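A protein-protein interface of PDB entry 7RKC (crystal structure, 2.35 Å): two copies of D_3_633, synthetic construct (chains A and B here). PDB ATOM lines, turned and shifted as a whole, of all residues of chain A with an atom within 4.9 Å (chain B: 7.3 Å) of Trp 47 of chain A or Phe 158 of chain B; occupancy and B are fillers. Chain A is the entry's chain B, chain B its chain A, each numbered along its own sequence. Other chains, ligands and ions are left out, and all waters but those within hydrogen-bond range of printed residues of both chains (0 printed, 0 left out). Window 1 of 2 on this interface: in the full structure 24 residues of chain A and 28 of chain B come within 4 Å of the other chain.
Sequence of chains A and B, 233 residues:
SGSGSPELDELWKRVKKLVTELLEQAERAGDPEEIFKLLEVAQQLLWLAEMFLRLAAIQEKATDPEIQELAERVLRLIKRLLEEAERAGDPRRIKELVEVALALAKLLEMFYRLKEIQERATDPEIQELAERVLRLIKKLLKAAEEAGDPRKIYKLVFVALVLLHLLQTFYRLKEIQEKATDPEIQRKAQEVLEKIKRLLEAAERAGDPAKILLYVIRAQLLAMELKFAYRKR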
ATOM      1  N   PHE A  36      16.451  24.392  28.371  1.00  0.00           N
ATOM      2  CA  PHE A  36      17.531  23.411  28.358  1.00  0.00           C
ATOM      3  C   PHE A  36      17.790  22.863  29.756  1.00  0.00           C
ATOM      4  O   PHE A  36      18.065  21.667  29.917  1.00  0.00           O
ATOM      5  CB  PHE A  36      18.804  24.035  27.782  1.00  0.00           C
ATOM      6  CG  PHE A  36      19.870  23.032  27.430  1.00  0.00           C
ATOM      7  CD1 PHE A  36      20.691  22.496  28.411  1.00  0.00           C
ATOM      8  CD2 PHE A  36      20.049  22.628  26.119  1.00  0.00           C
ATOM      9  CE1 PHE A  36      21.667  21.574  28.091  1.00  0.00           C
ATOM     10  CE2 PHE A  36      21.027  21.706  25.791  1.00  0.00           C
ATOM     11  CZ  PHE A  36      21.834  21.178  26.780  1.00  0.00           C
ATOM     12  N   GLU A  40      17.805  18.808  30.638  1.00  0.00           N
ATOM     13  CA  GLU A  40      18.986  18.072  31.078  1.00  0.00           C
ATOM     14  C   GLU A  40      18.692  17.282  32.347  1.00  0.00           C
ATOM     15  O   GLU A  40      19.216  16.176  32.531  1.00  0.00           O
ATOM     16  CB  GLU A  40      20.180  19.011  31.267  1.00  0.00           C
ATOM     17  CG  GLU A  40      19.954  20.228  32.132  1.00  0.00           C
ATOM     18  CD  GLU A  40      21.222  21.051  32.286  1.00  0.00           C
ATOM     19  OE1 GLU A  40      22.265  20.636  31.737  1.00  0.00           O
ATOM     20  OE2 GLU A  40      21.176  22.109  32.948  1.00  0.00           O
ATOM     21  N   GLN A  43      17.003  14.400  31.101  1.00  0.00           N
ATOM     22  CA  GLN A  43      17.982  13.501  30.499  1.00  0.00           C
ATOM     23  C   GLN A  43      18.740  12.715  31.562  1.00  0.00           C
ATOM     24  O   GLN A  43      19.034  11.530  31.372  1.00  0.00           O
ATOM     25  CB  GLN A  43      18.951  14.292  29.620  1.00  0.00           C
ATOM     26  CG  GLN A  43      19.956  13.421  28.897  1.00  0.00           C
ATOM     27  CD  GLN A  43      19.297  12.278  28.153  1.00  0.00           C
ATOM     28  OE1 GLN A  43      19.560  11.107  28.431  1.00  0.00           O
ATOM     29  NE2 GLN A  43      18.435  12.611  27.200  1.00  0.00           N
ATOM     30  N   GLN A  44      19.067  13.357  32.687  1.00  0.00           N
ATOM     31  CA  GLN A  44      19.750  12.649  33.764  1.00  0.00           C
ATOM     32  C   GLN A  44      18.863  11.575  34.380  1.00  0.00           C
ATOM     33  O   GLN A  44      19.363  10.524  34.797  1.00  0.00           O
ATOM     34  CB  GLN A  44      20.209  13.637  34.835  1.00  0.00           C
ATOM     35  N   LEU A  45      17.551  11.816  34.441  1.00  0.00           N
ATOM     36  CA  LEU A  45      16.635  10.810  34.967  1.00  0.00           C
ATOM     37  C   LEU A  45      16.571   9.590  34.056  1.00  0.00           C
ATOM     38  O   LEU A  45      16.510   8.452  34.538  1.00  0.00           O
ATOM     39  CB  LEU A  45      15.244  11.416  35.152  1.00  0.00           C
ATOM     40  CG  LEU A  45      14.995  12.193  36.445  1.00  0.00           C
ATOM     41  CD1 LEU A  45      13.762  13.069  36.305  1.00  0.00           C
ATOM     42  CD2 LEU A  45      14.845  11.235  37.615  1.00  0.00           C
ATOM     43  N   LEU A  46      16.581   9.805  32.739  1.00  0.00           N
ATOM     44  CA  LEU A  46      16.574   8.684  31.806  1.00  0.00           C
ATOM     45  C   LEU A  46      17.852   7.865  31.924  1.00  0.00           C
ATOM     46  O   LEU A  46      17.820   6.631  31.833  1.00  0.00           O
ATOM     47  CB  LEU A  46      16.394   9.187  30.374  1.00  0.00           C
ATOM     48  CG  LEU A  46      15.100   9.933  30.046  1.00  0.00           C
ATOM     49  CD1 LEU A  46      15.127  10.424  28.606  1.00  0.00           C
ATOM     50  CD2 LEU A  46      13.883   9.052  30.298  1.00  0.00           C
ATOM     51  N   TRP A  47      18.990   8.534  32.124  1.00  0.00           N
ATOM     52  CA  TRP A  47      20.242   7.814  32.325  1.00  0.00           C
ATOM     53  C   TRP A  47      20.218   7.030  33.631  1.00  0.00           C
ATOM     54  O   TRP A  47      20.763   5.924  33.706  1.00  0.00           O
ATOM     55  CB  TRP A  47      21.418   8.787  32.286  1.00  0.00           C
ATOM     56  CG  TRP A  47      21.882   9.069  30.890  1.00  0.00           C
ATOM     57  CD1 TRP A  47      21.839   8.214  29.828  1.00  0.00           C
ATOM     58  CD2 TRP A  47      22.448  10.290  30.400  1.00  0.00           C
ATOM     59  NE1 TRP A  47      22.348   8.824  28.707  1.00  0.00           N
ATOM     60  CE2 TRP A  47      22.729  10.098  29.032  1.00  0.00           C
ATOM     61  CE3 TRP A  47      22.748  11.524  30.984  1.00  0.00           C
ATOM     62  CZ2 TRP A  47      23.294  11.095  28.239  1.00  0.00           C
ATOM     63  CZ3 TRP A  47      23.309  12.512  30.195  1.00  0.00           C
ATOM     64  CH2 TRP A  47      23.576  12.292  28.838  1.00  0.00           C
ATOM     65  N   LEU A  48      19.593   7.589  34.671  1.00  0.00           N
ATOM     66  CA  LEU A  48      19.400   6.838  35.908  1.00  0.00           C
ATOM     67  C   LEU A  48      18.562   5.592  35.654  1.00  0.00           C
ATOM     68  O   LEU A  48      18.889   4.499  36.130  1.00  0.00           O
ATOM     69  CB  LEU A  48      18.746   7.730  36.963  1.00  0.00           C
ATOM     70  CG  LEU A  48      18.343   7.049  38.274  1.00  0.00           C
ATOM     71  CD1 LEU A  48      19.570   6.755  39.125  1.00  0.00           C
ATOM     72  CD2 LEU A  48      17.343   7.901  39.039  1.00  0.00           C
ATOM     73  N   ALA A  49      17.468   5.743  34.903  1.00  0.00           N
ATOM     74  CA  ALA A  49      16.672   4.588  34.500  1.00  0.00           C
ATOM     75  C   ALA A  49      17.482   3.654  33.613  1.00  0.00           C
ATOM     76  O   ALA A  49      17.335   2.427  33.686  1.00  0.00           O
ATOM     77  CB  ALA A  49      15.404   5.047  33.785  1.00  0.00           C
ATOM     78  N   GLU A  50      18.338   4.219  32.758  1.00  0.00           N
ATOM     79  CA  GLU A  50      19.216   3.398  31.931  1.00  0.00           C
ATOM     80  C   GLU A  50      20.187   2.598  32.787  1.00  0.00           C
ATOM     81  O   GLU A  50      20.544   1.469  32.434  1.00  0.00           O
ATOM     82  CB  GLU A  50      19.972   4.279  30.934  1.00  0.00           C
ATOM     83  CG  GLU A  50      20.826   3.512  29.934  1.00  0.00           C
ATOM     84  CD  GLU A  50      20.023   2.975  28.764  1.00  0.00           C
ATOM     85  OE1 GLU A  50      18.776   2.961  28.843  1.00  0.00           O
ATOM     86  OE2 GLU A  50      20.642   2.567  27.758  1.00  0.00           O
ATOM     87  N   MET A  51      20.622   3.164  33.915  1.00  0.00           N
ATOM     88  CA  MET A  51      21.459   2.410  34.841  1.00  0.00           C
ATOM     89  C   MET A  51      20.647   1.358  35.584  1.00  0.00           C
ATOM     90  O   MET A  51      21.190   0.314  35.965  1.00  0.00           O
ATOM     91  CB  MET A  51      22.146   3.358  35.824  1.00  0.00           C
ATOM     92  CG  MET A  51      23.090   4.350  35.158  1.00  0.00           C
ATOM     93  SD  MET A  51      24.037   5.330  36.337  1.00  0.00           S
ATOM     94  CE  MET A  51      25.239   4.120  36.880  1.00  0.00           C
ATOM     95  N   LEU A 102      22.254   9.171  40.841  1.00  0.00           N
ATOM     96  CA  LEU A 102      23.196   8.767  39.804  1.00  0.00           C
ATOM     97  C   LEU A 102      24.510   8.303  40.415  1.00  0.00           C
ATOM     98  O   LEU A 102      25.088   7.301  39.978  1.00  0.00           O
ATOM     99  CB  LEU A 102      23.429   9.922  38.832  1.00  0.00           C
ATOM    100  CG  LEU A 102      22.372  10.082  37.738  1.00  0.00           C
ATOM    101  CD1 LEU A 102      22.611  11.349  36.933  1.00  0.00           C
ATOM    102  CD2 LEU A 102      22.354   8.859  36.835  1.00  0.00           C
ATOM    103  N   ALA B 103      32.531  15.817  29.671  1.00  0.00           N
ATOM    104  CA  ALA B 103      31.501  15.475  28.695  1.00  0.00           C
ATOM    105  C   ALA B 103      32.112  15.203  27.327  1.00  0.00           C
ATOM    106  O   ALA B 103      31.638  14.333  26.588  1.00  0.00           O
ATOM    107  CB  ALA B 103      30.462  16.593  28.610  1.00  0.00           C
ATOM    108  N   LEU B 104      33.163  15.945  26.971  1.00  0.00           N
ATOM    109  CA  LEU B 104      33.867  15.675  25.723  1.00  0.00           C
ATOM    110  C   LEU B 104      34.547  14.313  25.764  1.00  0.00           C
ATOM    111  O   LEU B 104      34.566  13.591  24.760  1.00  0.00           O
ATOM    112  CB  LEU B 104      34.883  16.781  25.443  1.00  0.00           C
ATOM    113  CG  LEU B 104      34.300  18.108  24.957  1.00  0.00           C
ATOM    114  CD1 LEU B 104      35.279  19.251  25.200  1.00  0.00           C
ATOM    115  CD2 LEU B 104      33.935  18.011  23.485  1.00  0.00           C
ATOM    116  N   LEU B 107      31.868  11.937  25.308  1.00  0.00           N
ATOM    117  CA  LEU B 107      31.458  11.991  23.909  1.00  0.00           C
ATOM    118  C   LEU B 107      32.426  11.223  23.019  1.00  0.00           C
ATOM    119  O   LEU B 107      32.004  10.505  22.104  1.00  0.00           O
ATOM    120  CB  LEU B 107      31.349  13.445  23.449  1.00  0.00           C
ATOM    121  CG  LEU B 107      30.940  13.650  21.988  1.00  0.00           C
ATOM    122  CD1 LEU B 107      29.449  13.414  21.812  1.00  0.00           C
ATOM    123  CD2 LEU B 107      31.329  15.038  21.504  1.00  0.00           C
ATOM    124  N   MET B 110      31.854   7.447  23.539  1.00  0.00           N
ATOM    125  CA  MET B 110      30.650   6.982  22.857  1.00  0.00           C
ATOM    126  C   MET B 110      30.837   6.945  21.345  1.00  0.00           C
ATOM    127  O   MET B 110      30.257   6.084  20.673  1.00  0.00           O
ATOM    128  CB  MET B 110      29.460   7.867  23.227  1.00  0.00           C
ATOM    129  CG  MET B 110      28.894   7.589  24.611  1.00  0.00           C
ATOM    130  SD  MET B 110      27.208   8.193  24.813  1.00  0.00           S
ATOM    131  N   LEU B 140      27.368  20.298  15.650  1.00  0.00           N
ATOM    132  CA  LEU B 140      27.368  20.789  17.024  1.00  0.00           C
ATOM    133  C   LEU B 140      28.786  20.923  17.561  1.00  0.00           C
ATOM    134  O   LEU B 140      29.084  21.848  18.326  1.00  0.00           O
ATOM    135  CB  LEU B 140      26.552  19.856  17.921  1.00  0.00           C
ATOM    136  CG  LEU B 140      25.061  19.689  17.633  1.00  0.00           C
ATOM    137  CD1 LEU B 140      24.538  18.433  18.313  1.00  0.00           C
ATOM    138  CD2 LEU B 140      24.278  20.913  18.082  1.00  0.00           C
ATOM    139  N   ARG B 151      29.396  27.351  29.046  1.00  0.00           N
ATOM    140  CA  ARG B 151      28.032  26.836  29.097  1.00  0.00           C
ATOM    141  C   ARG B 151      27.504  26.546  27.699  1.00  0.00           C
ATOM    142  O   ARG B 151      26.847  25.523  27.475  1.00  0.00           O
ATOM    143  CB  ARG B 151      27.126  27.832  29.821  1.00  0.00           C
ATOM    144  CG  ARG B 151      25.643  27.512  29.733  1.00  0.00           C
ATOM    145  CD  ARG B 151      25.311  26.221  30.460  1.00  0.00           C
ATOM    146  NE  ARG B 151      23.876  25.955  30.465  1.00  0.00           N
ATOM    147  CZ  ARG B 151      23.326  24.837  30.924  1.00  0.00           C
ATOM    148  NH1 ARG B 151      24.093  23.873  31.419  1.00  0.00           N
ATOM    149  NH2 ARG B 151      22.011  24.680  30.891  1.00  0.00           N
ATOM    150  N   LYS B 152      27.790  27.432  26.741  1.00  0.00           N
ATOM    151  CA  LYS B 152      27.360  27.201  25.366  1.00  0.00           C
ATOM    152  C   LYS B 152      28.046  25.977  24.774  1.00  0.00           C
ATOM    153  O   LYS B 152      27.431  25.220  24.014  1.00  0.00           O
ATOM    154  CB  LYS B 152      27.639  28.440  24.516  1.00  0.00           C
ATOM    155  N   ILE B 153      29.324  25.771  25.101  1.00  0.00           N
ATOM    156  CA  ILE B 153      30.016  24.574  24.637  1.00  0.00           C
ATOM    157  C   ILE B 153      29.413  23.328  25.273  1.00  0.00           C
ATOM    158  O   ILE B 153      29.194  22.315  24.598  1.00  0.00           O
ATOM    159  CB  ILE B 153      31.525  24.676  24.926  1.00  0.00           C
ATOM    160  CG1 ILE B 153      32.120  25.916  24.254  1.00  0.00           C
ATOM    161  CG2 ILE B 153      32.244  23.418  24.461  1.00  0.00           C
ATOM    162  CD1 ILE B 153      33.548  26.201  24.668  1.00  0.00           C
ATOM    163  N   TYR B 154      29.133  23.383  26.578  1.00  0.00           N
ATOM    164  CA  TYR B 154      28.590  22.219  27.271  1.00  0.00           C
ATOM    165  C   TYR B 154      27.243  21.807  26.691  1.00  0.00           C
ATOM    166  O   TYR B 154      26.999  20.622  26.441  1.00  0.00           O
ATOM    167  CB  TYR B 154      28.460  22.503  28.767  1.00  0.00           C
ATOM    168  CG  TYR B 154      27.779  21.385  29.522  1.00  0.00           C
ATOM    169  CD1 TYR B 154      28.481  20.248  29.900  1.00  0.00           C
ATOM    170  CD2 TYR B 154      26.428  21.457  29.844  1.00  0.00           C
ATOM    171  CE1 TYR B 154      27.862  19.219  30.582  1.00  0.00           C
ATOM    172  CE2 TYR B 154      25.801  20.433  30.526  1.00  0.00           C
ATOM    173  CZ  TYR B 154      26.522  19.317  30.893  1.00  0.00           C
ATOM    174  OH  TYR B 154      25.903  18.293  31.573  1.00  0.00           O
ATOM    175  N   LYS B 155      26.350  22.779  26.480  1.00  0.00           N
ATOM    176  CA  LYS B 155      25.024  22.465  25.954  1.00  0.00           C
ATOM    177  C   LYS B 155      25.111  21.787  24.594  1.00  0.00           C
ATOM    178  O   LYS B 155      24.356  20.849  24.309  1.00  0.00           O
ATOM    179  CB  LYS B 155      24.182  23.740  25.862  1.00  0.00           C
ATOM    180  CG  LYS B 155      23.870  24.382  27.203  1.00  0.00           C
ATOM    181  CD  LYS B 155      23.305  25.784  27.024  1.00  0.00           C
ATOM    182  CE  LYS B 155      21.969  25.754  26.301  1.00  0.00           C
ATOM    183  NZ  LYS B 155      21.432  27.123  26.067  1.00  0.00           N
ATOM    184  N   LEU B 156      26.030  22.241  23.741  1.00  0.00           N
ATOM    185  CA  LEU B 156      26.158  21.650  22.413  1.00  0.00           C
ATOM    186  C   LEU B 156      26.830  20.286  22.477  1.00  0.00           C
ATOM    187  O   LEU B 156      26.465  19.371  21.730  1.00  0.00           O
ATOM    188  CB  LEU B 156      26.917  22.600  21.489  1.00  0.00           C
ATOM    189  CG  LEU B 156      26.119  23.841  21.073  1.00  0.00           C
ATOM    190  CD1 LEU B 156      26.527  24.301  19.692  1.00  0.00           C
ATOM    191  CD2 LEU B 156      24.619  23.579  21.119  1.00  0.00           C
ATOM    192  N   VAL B 157      27.818  20.129  23.360  1.00  0.00           N
ATOM    193  CA  VAL B 157      28.428  18.817  23.545  1.00  0.00           C
ATOM    194  C   VAL B 157      27.443  17.875  24.225  1.00  0.00           C
ATOM    195  O   VAL B 157      27.430  16.668  23.947  1.00  0.00           O
ATOM    196  CB  VAL B 157      29.741  18.950  24.338  1.00  0.00           C
ATOM    197  CG1 VAL B 157      30.297  17.583  24.708  1.00  0.00           C
ATOM    198  CG2 VAL B 157      30.761  19.739  23.533  1.00  0.00           C
ATOM    199  N   PHE B 158      26.597  18.405  25.111  1.00  0.00           N
ATOM    200  CA  PHE B 158      25.571  17.584  25.746  1.00  0.00           C
ATOM    201  C   PHE B 158      24.585  17.041  24.719  1.00  0.00           C
ATOM    202  O   PHE B 158      24.209  15.866  24.769  1.00  0.00           O
ATOM    203  CB  PHE B 158      24.838  18.392  26.816  1.00  0.00           C
ATOM    204  CG  PHE B 158      23.935  17.568  27.685  1.00  0.00           C
ATOM    205  CD1 PHE B 158      24.461  16.745  28.668  1.00  0.00           C
ATOM    206  CD2 PHE B 158      22.562  17.611  27.518  1.00  0.00           C
ATOM    207  CE1 PHE B 158      23.632  15.983  29.468  1.00  0.00           C
ATOM    208  CE2 PHE B 158      21.728  16.852  28.316  1.00  0.00           C
ATOM    209  CZ  PHE B 158      22.265  16.037  29.293  1.00  0.00           C
ATOM    210  N   VAL B 159      24.151  17.888  23.782  1.00  0.00           N
ATOM    211  CA  VAL B 159      23.216  17.442  22.753  1.00  0.00           C
ATOM    212  C   VAL B 159      23.880  16.424  21.831  1.00  0.00           C
ATOM    213  O   VAL B 159      23.251  15.448  21.406  1.00  0.00           O
ATOM    214  CB  VAL B 159      22.667  18.650  21.971  1.00  0.00           C
ATOM    215  CG1 VAL B 159      21.872  18.188  20.766  1.00  0.00           C
ATOM    216  CG2 VAL B 159      21.804  19.515  22.876  1.00  0.00           C
ATOM    217  N   ALA B 160      25.159  16.630  21.510  1.00  0.00           N
ATOM    218  CA  ALA B 160      25.885  15.636  20.728  1.00  0.00           C
ATOM    219  C   ALA B 160      25.996  14.315  21.478  1.00  0.00           C
ATOM    220  O   ALA B 160      25.977  13.245  20.862  1.00  0.00           O
ATOM    221  CB  ALA B 160      27.273  16.161  20.362  1.00  0.00           C
ATOM    222  N   LEU B 161      26.118  14.375  22.806  1.00  0.00           N
ATOM    223  CA  LEU B 161      26.224  13.160  23.609  1.00  0.00           C
ATOM    224  C   LEU B 161      24.941  12.338  23.549  1.00  0.00           C
ATOM    225  O   LEU B 161      24.985  11.116  23.358  1.00  0.00           O
ATOM    226  CB  LEU B 161      26.563  13.528  25.054  1.00  0.00           C
ATOM    227  CG  LEU B 161      26.962  12.401  26.006  1.00  0.00           C
ATOM    228  CD1 LEU B 161      28.187  11.672  25.487  1.00  0.00           C
ATOM    229  CD2 LEU B 161      27.213  12.953  27.401  1.00  0.00           C
ATOM    230  N   VAL B 162      23.785  12.988  23.713  1.00  0.00           N
ATOM    231  CA  VAL B 162      22.520  12.257  23.694  1.00  0.00           C
ATOM    232  C   VAL B 162      22.212  11.736  22.296  1.00  0.00           C
ATOM    233  O   VAL B 162      21.575  10.686  22.145  1.00  0.00           O
ATOM    234  CB  VAL B 162      21.375  13.131  24.247  1.00  0.00           C
ATOM    235  CG1 VAL B 162      21.727  13.651  25.633  1.00  0.00           C
ATOM    236  CG2 VAL B 162      21.055  14.283  23.309  1.00  0.00           C
ATOM    237  N   LEU B 163      22.639  12.456  21.255  1.00  0.00           N
ATOM    238  CA  LEU B 163      22.464  11.965  19.892  1.00  0.00           C
ATOM    239  C   LEU B 163      23.218  10.658  19.675  1.00  0.00           C
ATOM    240  O   LEU B 163      22.704   9.735  19.033  1.00  0.00           O
ATOM    241  CB  LEU B 163      22.926  13.022  18.888  1.00  0.00           C
ATOM    242  CG  LEU B 163      21.930  14.130  18.544  1.00  0.00           C
ATOM    243  CD1 LEU B 163      22.577  15.169  17.640  1.00  0.00           C
ATOM    244  CD2 LEU B 163      20.684  13.550  17.897  1.00  0.00           C
ATOM    245  N   LEU B 164      24.443  10.563  20.201  1.00  0.00           N
ATOM    246  CA  LEU B 164      25.203   9.323  20.079  1.00  0.00           C
ATOM    247  C   LEU B 164      24.526   8.183  20.828  1.00  0.00           C
ATOM    248  O   LEU B 164      24.497   7.044  20.345  1.00  0.00           O
ATOM    249  CB  LEU B 164      26.627   9.526  20.596  1.00  0.00           C
ATOM    250  CG  LEU B 164      27.699   9.872  19.561  1.00  0.00           C
ATOM    251  CD1 LEU B 164      29.056  10.045  20.226  1.00  0.00           C
ATOM    252  CD2 LEU B 164      27.760   8.813  18.473  1.00  0.00           C
ATOM    253  N   HIS B 165      23.981   8.466  22.012  1.00  0.00           N
ATOM    254  CA  HIS B 165      23.267   7.433  22.757  1.00  0.00           C
ATOM    255  C   HIS B 165      21.978   7.034  22.051  1.00  0.00           C
ATOM    256  O   HIS B 165      21.617   5.851  22.034  1.00  0.00           O
ATOM    257  CB  HIS B 165      22.977   7.907  24.180  1.00  0.00           C
ATOM    258  CG  HIS B 165      22.682   6.792  25.133  1.00  0.00           C
ATOM    259  ND1 HIS B 165      23.615   5.835  25.473  1.00  0.00           N
ATOM    260  CD2 HIS B 165      21.556   6.473  25.816  1.00  0.00           C
ATOM    261  CE1 HIS B 165      23.080   4.980  26.324  1.00  0.00           C
ATOM    262  NE2 HIS B 165      21.826   5.346  26.549  1.00  0.00           N
ATOM    263  N   LEU B 213      17.258  18.538  21.769  1.00  0.00           N
ATOM    264  CA  LEU B 213      17.301  17.787  23.019  1.00  0.00           C
ATOM    265  C   LEU B 213      15.928  17.237  23.387  1.00  0.00           C
ATOM    266  O   LEU B 213      15.818  16.114  23.893  1.00  0.00           O
ATOM    267  CB  LEU B 213      17.846  18.672  24.140  1.00  0.00           C
ATOM    268  CG  LEU B 213      18.006  18.033  25.519  1.00  0.00           C
ATOM    269  CD1 LEU B 213      18.851  16.772  25.431  1.00  0.00           C
ATOM    270  CD2 LEU B 213      18.621  19.026  26.494  1.00  0.00           C
ATOM    271  N   ILE B 217      14.905  13.242  23.908  1.00  0.00           N
ATOM    272  CA  ILE B 217      14.323  12.757  25.155  1.00  0.00           C
ATOM    273  C   ILE B 217      12.967  12.114  24.891  1.00  0.00           C
ATOM    274  O   ILE B 217      12.608  11.108  25.517  1.00  0.00           O
ATOM    275  CB  ILE B 217      14.230  13.899  26.182  1.00  0.00           C
ATOM    276  CG1 ILE B 217      15.633  14.323  26.619  1.00  0.00           C
ATOM    277  CG2 ILE B 217      13.432  13.460  27.390  1.00  0.00           C
ATOM    278  CD1 ILE B 217      15.681  15.680  27.265  1.00  0.00           C
ATOM    279  N   GLN B 220      13.917   8.666  23.565  1.00  0.00           N
ATOM    280  CA  GLN B 220      14.400   7.737  24.578  1.00  0.00           C
ATOM    281  C   GLN B 220      13.277   7.290  25.503  1.00  0.00           C
ATOM    282  O   GLN B 220      13.293   6.153  25.989  1.00  0.00           O
ATOM    283  CB  GLN B 220      15.540   8.371  25.376  1.00  0.00           C
ATOM    284  CG  GLN B 220      16.757   8.743  24.536  1.00  0.00           C
ATOM    285  CD  GLN B 220      17.596   7.543  24.125  1.00  0.00           C
ATOM    286  OE1 GLN B 220      17.134   6.402  24.144  1.00  0.00           O
ATOM    287  NE2 GLN B 220      18.841   7.803  23.747  1.00  0.00           N
ATOM    288  N   MET B 224      12.870   3.402  25.969  1.00  0.00           N
ATOM    289  CA  MET B 224      13.070   2.757  27.261  1.00  0.00           C
ATOM    290  C   MET B 224      11.785   2.142  27.800  1.00  0.00           C
ATOM    291  O   MET B 224      11.844   1.154  28.541  1.00  0.00           O
ATOM    292  CB  MET B 224      13.648   3.749  28.270  1.00  0.00           C
ATOM    293  CG  MET B 224      15.156   3.629  28.442  1.00  0.00           C
ATOM    294  SD  MET B 224      15.866   4.974  29.402  1.00  0.00           S
ATOM    295  CE  MET B 224      15.395   6.369  28.389  1.00  0.00           C
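NH2 of Arg 151 of chain B lies within salt-bridge range of OE2 of Glu 40 of chain A, at 3.4 Å. The backbone carbonyl oxygen of Leu 46 of chain A sits close to the side-chain sulfur of Met 224 of chain B (3.5 Å). A ring nitrogen (NE2) of His 165 of chain B sits close to the side-chain carboxylate (OE2) of Glu 50 of chain A (3.3 Å). The side-chain carboxylate (OE1) of Glu 50 of chain A lies close to the side-chain sulfur (SD) of Met 224 of chain B, at 3.6 Å.
Among the printed residues, pairs that only touch across the chains: Phe 36 of chain A with Arg 151 of chain B, Phe 36 of chain A with Lys 155 of chain B, Phe 36 of chain A with Phe 158 of chain B, Phe 36 of chain A with Val 159 of chain B, Phe 36 of chain A with Leu 213 of chain B, Glu 40 of chain A with Tyr 154 of chain B, Glu 40 of chain A with Phe 158 of chain B, Gln 43 of chain A with Phe 158 of chain B, Gln 43 of chain A with Val 162 of chain B, Gln 43 of chain A with Ile 217 of chain B, Leu 46 of chain A with Ile 217 of chain B, Leu 46 of chain A with Gln 220 of chain B, Trp 47 of chain A with Phe 158 of chain B, Trp 47 of chain A with Leu 161 of chain B, Trp 47 of chain A with Val 162 of chain B and Trp 47 of chain A with His 165 of chain B.
Of the printed residues of chain B, Glu 40 of chain A touches Arg 151 (3.4 Å), Tyr 154 (3.7 Å) and Phe 158 (3.97 Å). Of the printed residues of chain B, Trp 47 of chain A touches Phe 158 (3.6 Å), Leu 161 (3.97 Å), Val 162 (3.9 Å) and His 165 (3.8 Å). Leu 140 of chain B touches none of the printed residues of chain A. Printed residues of chain A within 4 Å of Lys 155 of chain B: Phe 36. Phe 158 of chain B touches four residues of chain A. Of the printed residues of chain A, Val 162 of chain B touches Gln 43 and Trp 47. Printed residues of chain A within 4 Å of Met 224 of chain B: Leu 46 and Glu 50. The nearest residue of chain B that does not touch Trp 47 of chain A is Met 224 of chain B (5.5 Å). The nearest printed residue of chain A that does not touch Phe 158 of chain B is Gln 44 of chain A (5.4 Å).
Of the 24 printed residues of chain B, 12 touch a printed residue of chain A. Among the printed residues, 20 pairs touch across the chains. Among the printed residues, Asp or Glu carboxylates within 4 Å of a Lys or Arg side-chain nitrogen of the other chain: Glu 40 of chain A with Arg 151 of chain B (3.4 Å).
No position is printed for both chains. Of the 20 pairs that touch across the chains among the printed residues, none has its exchanged pair printed and touching as well.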
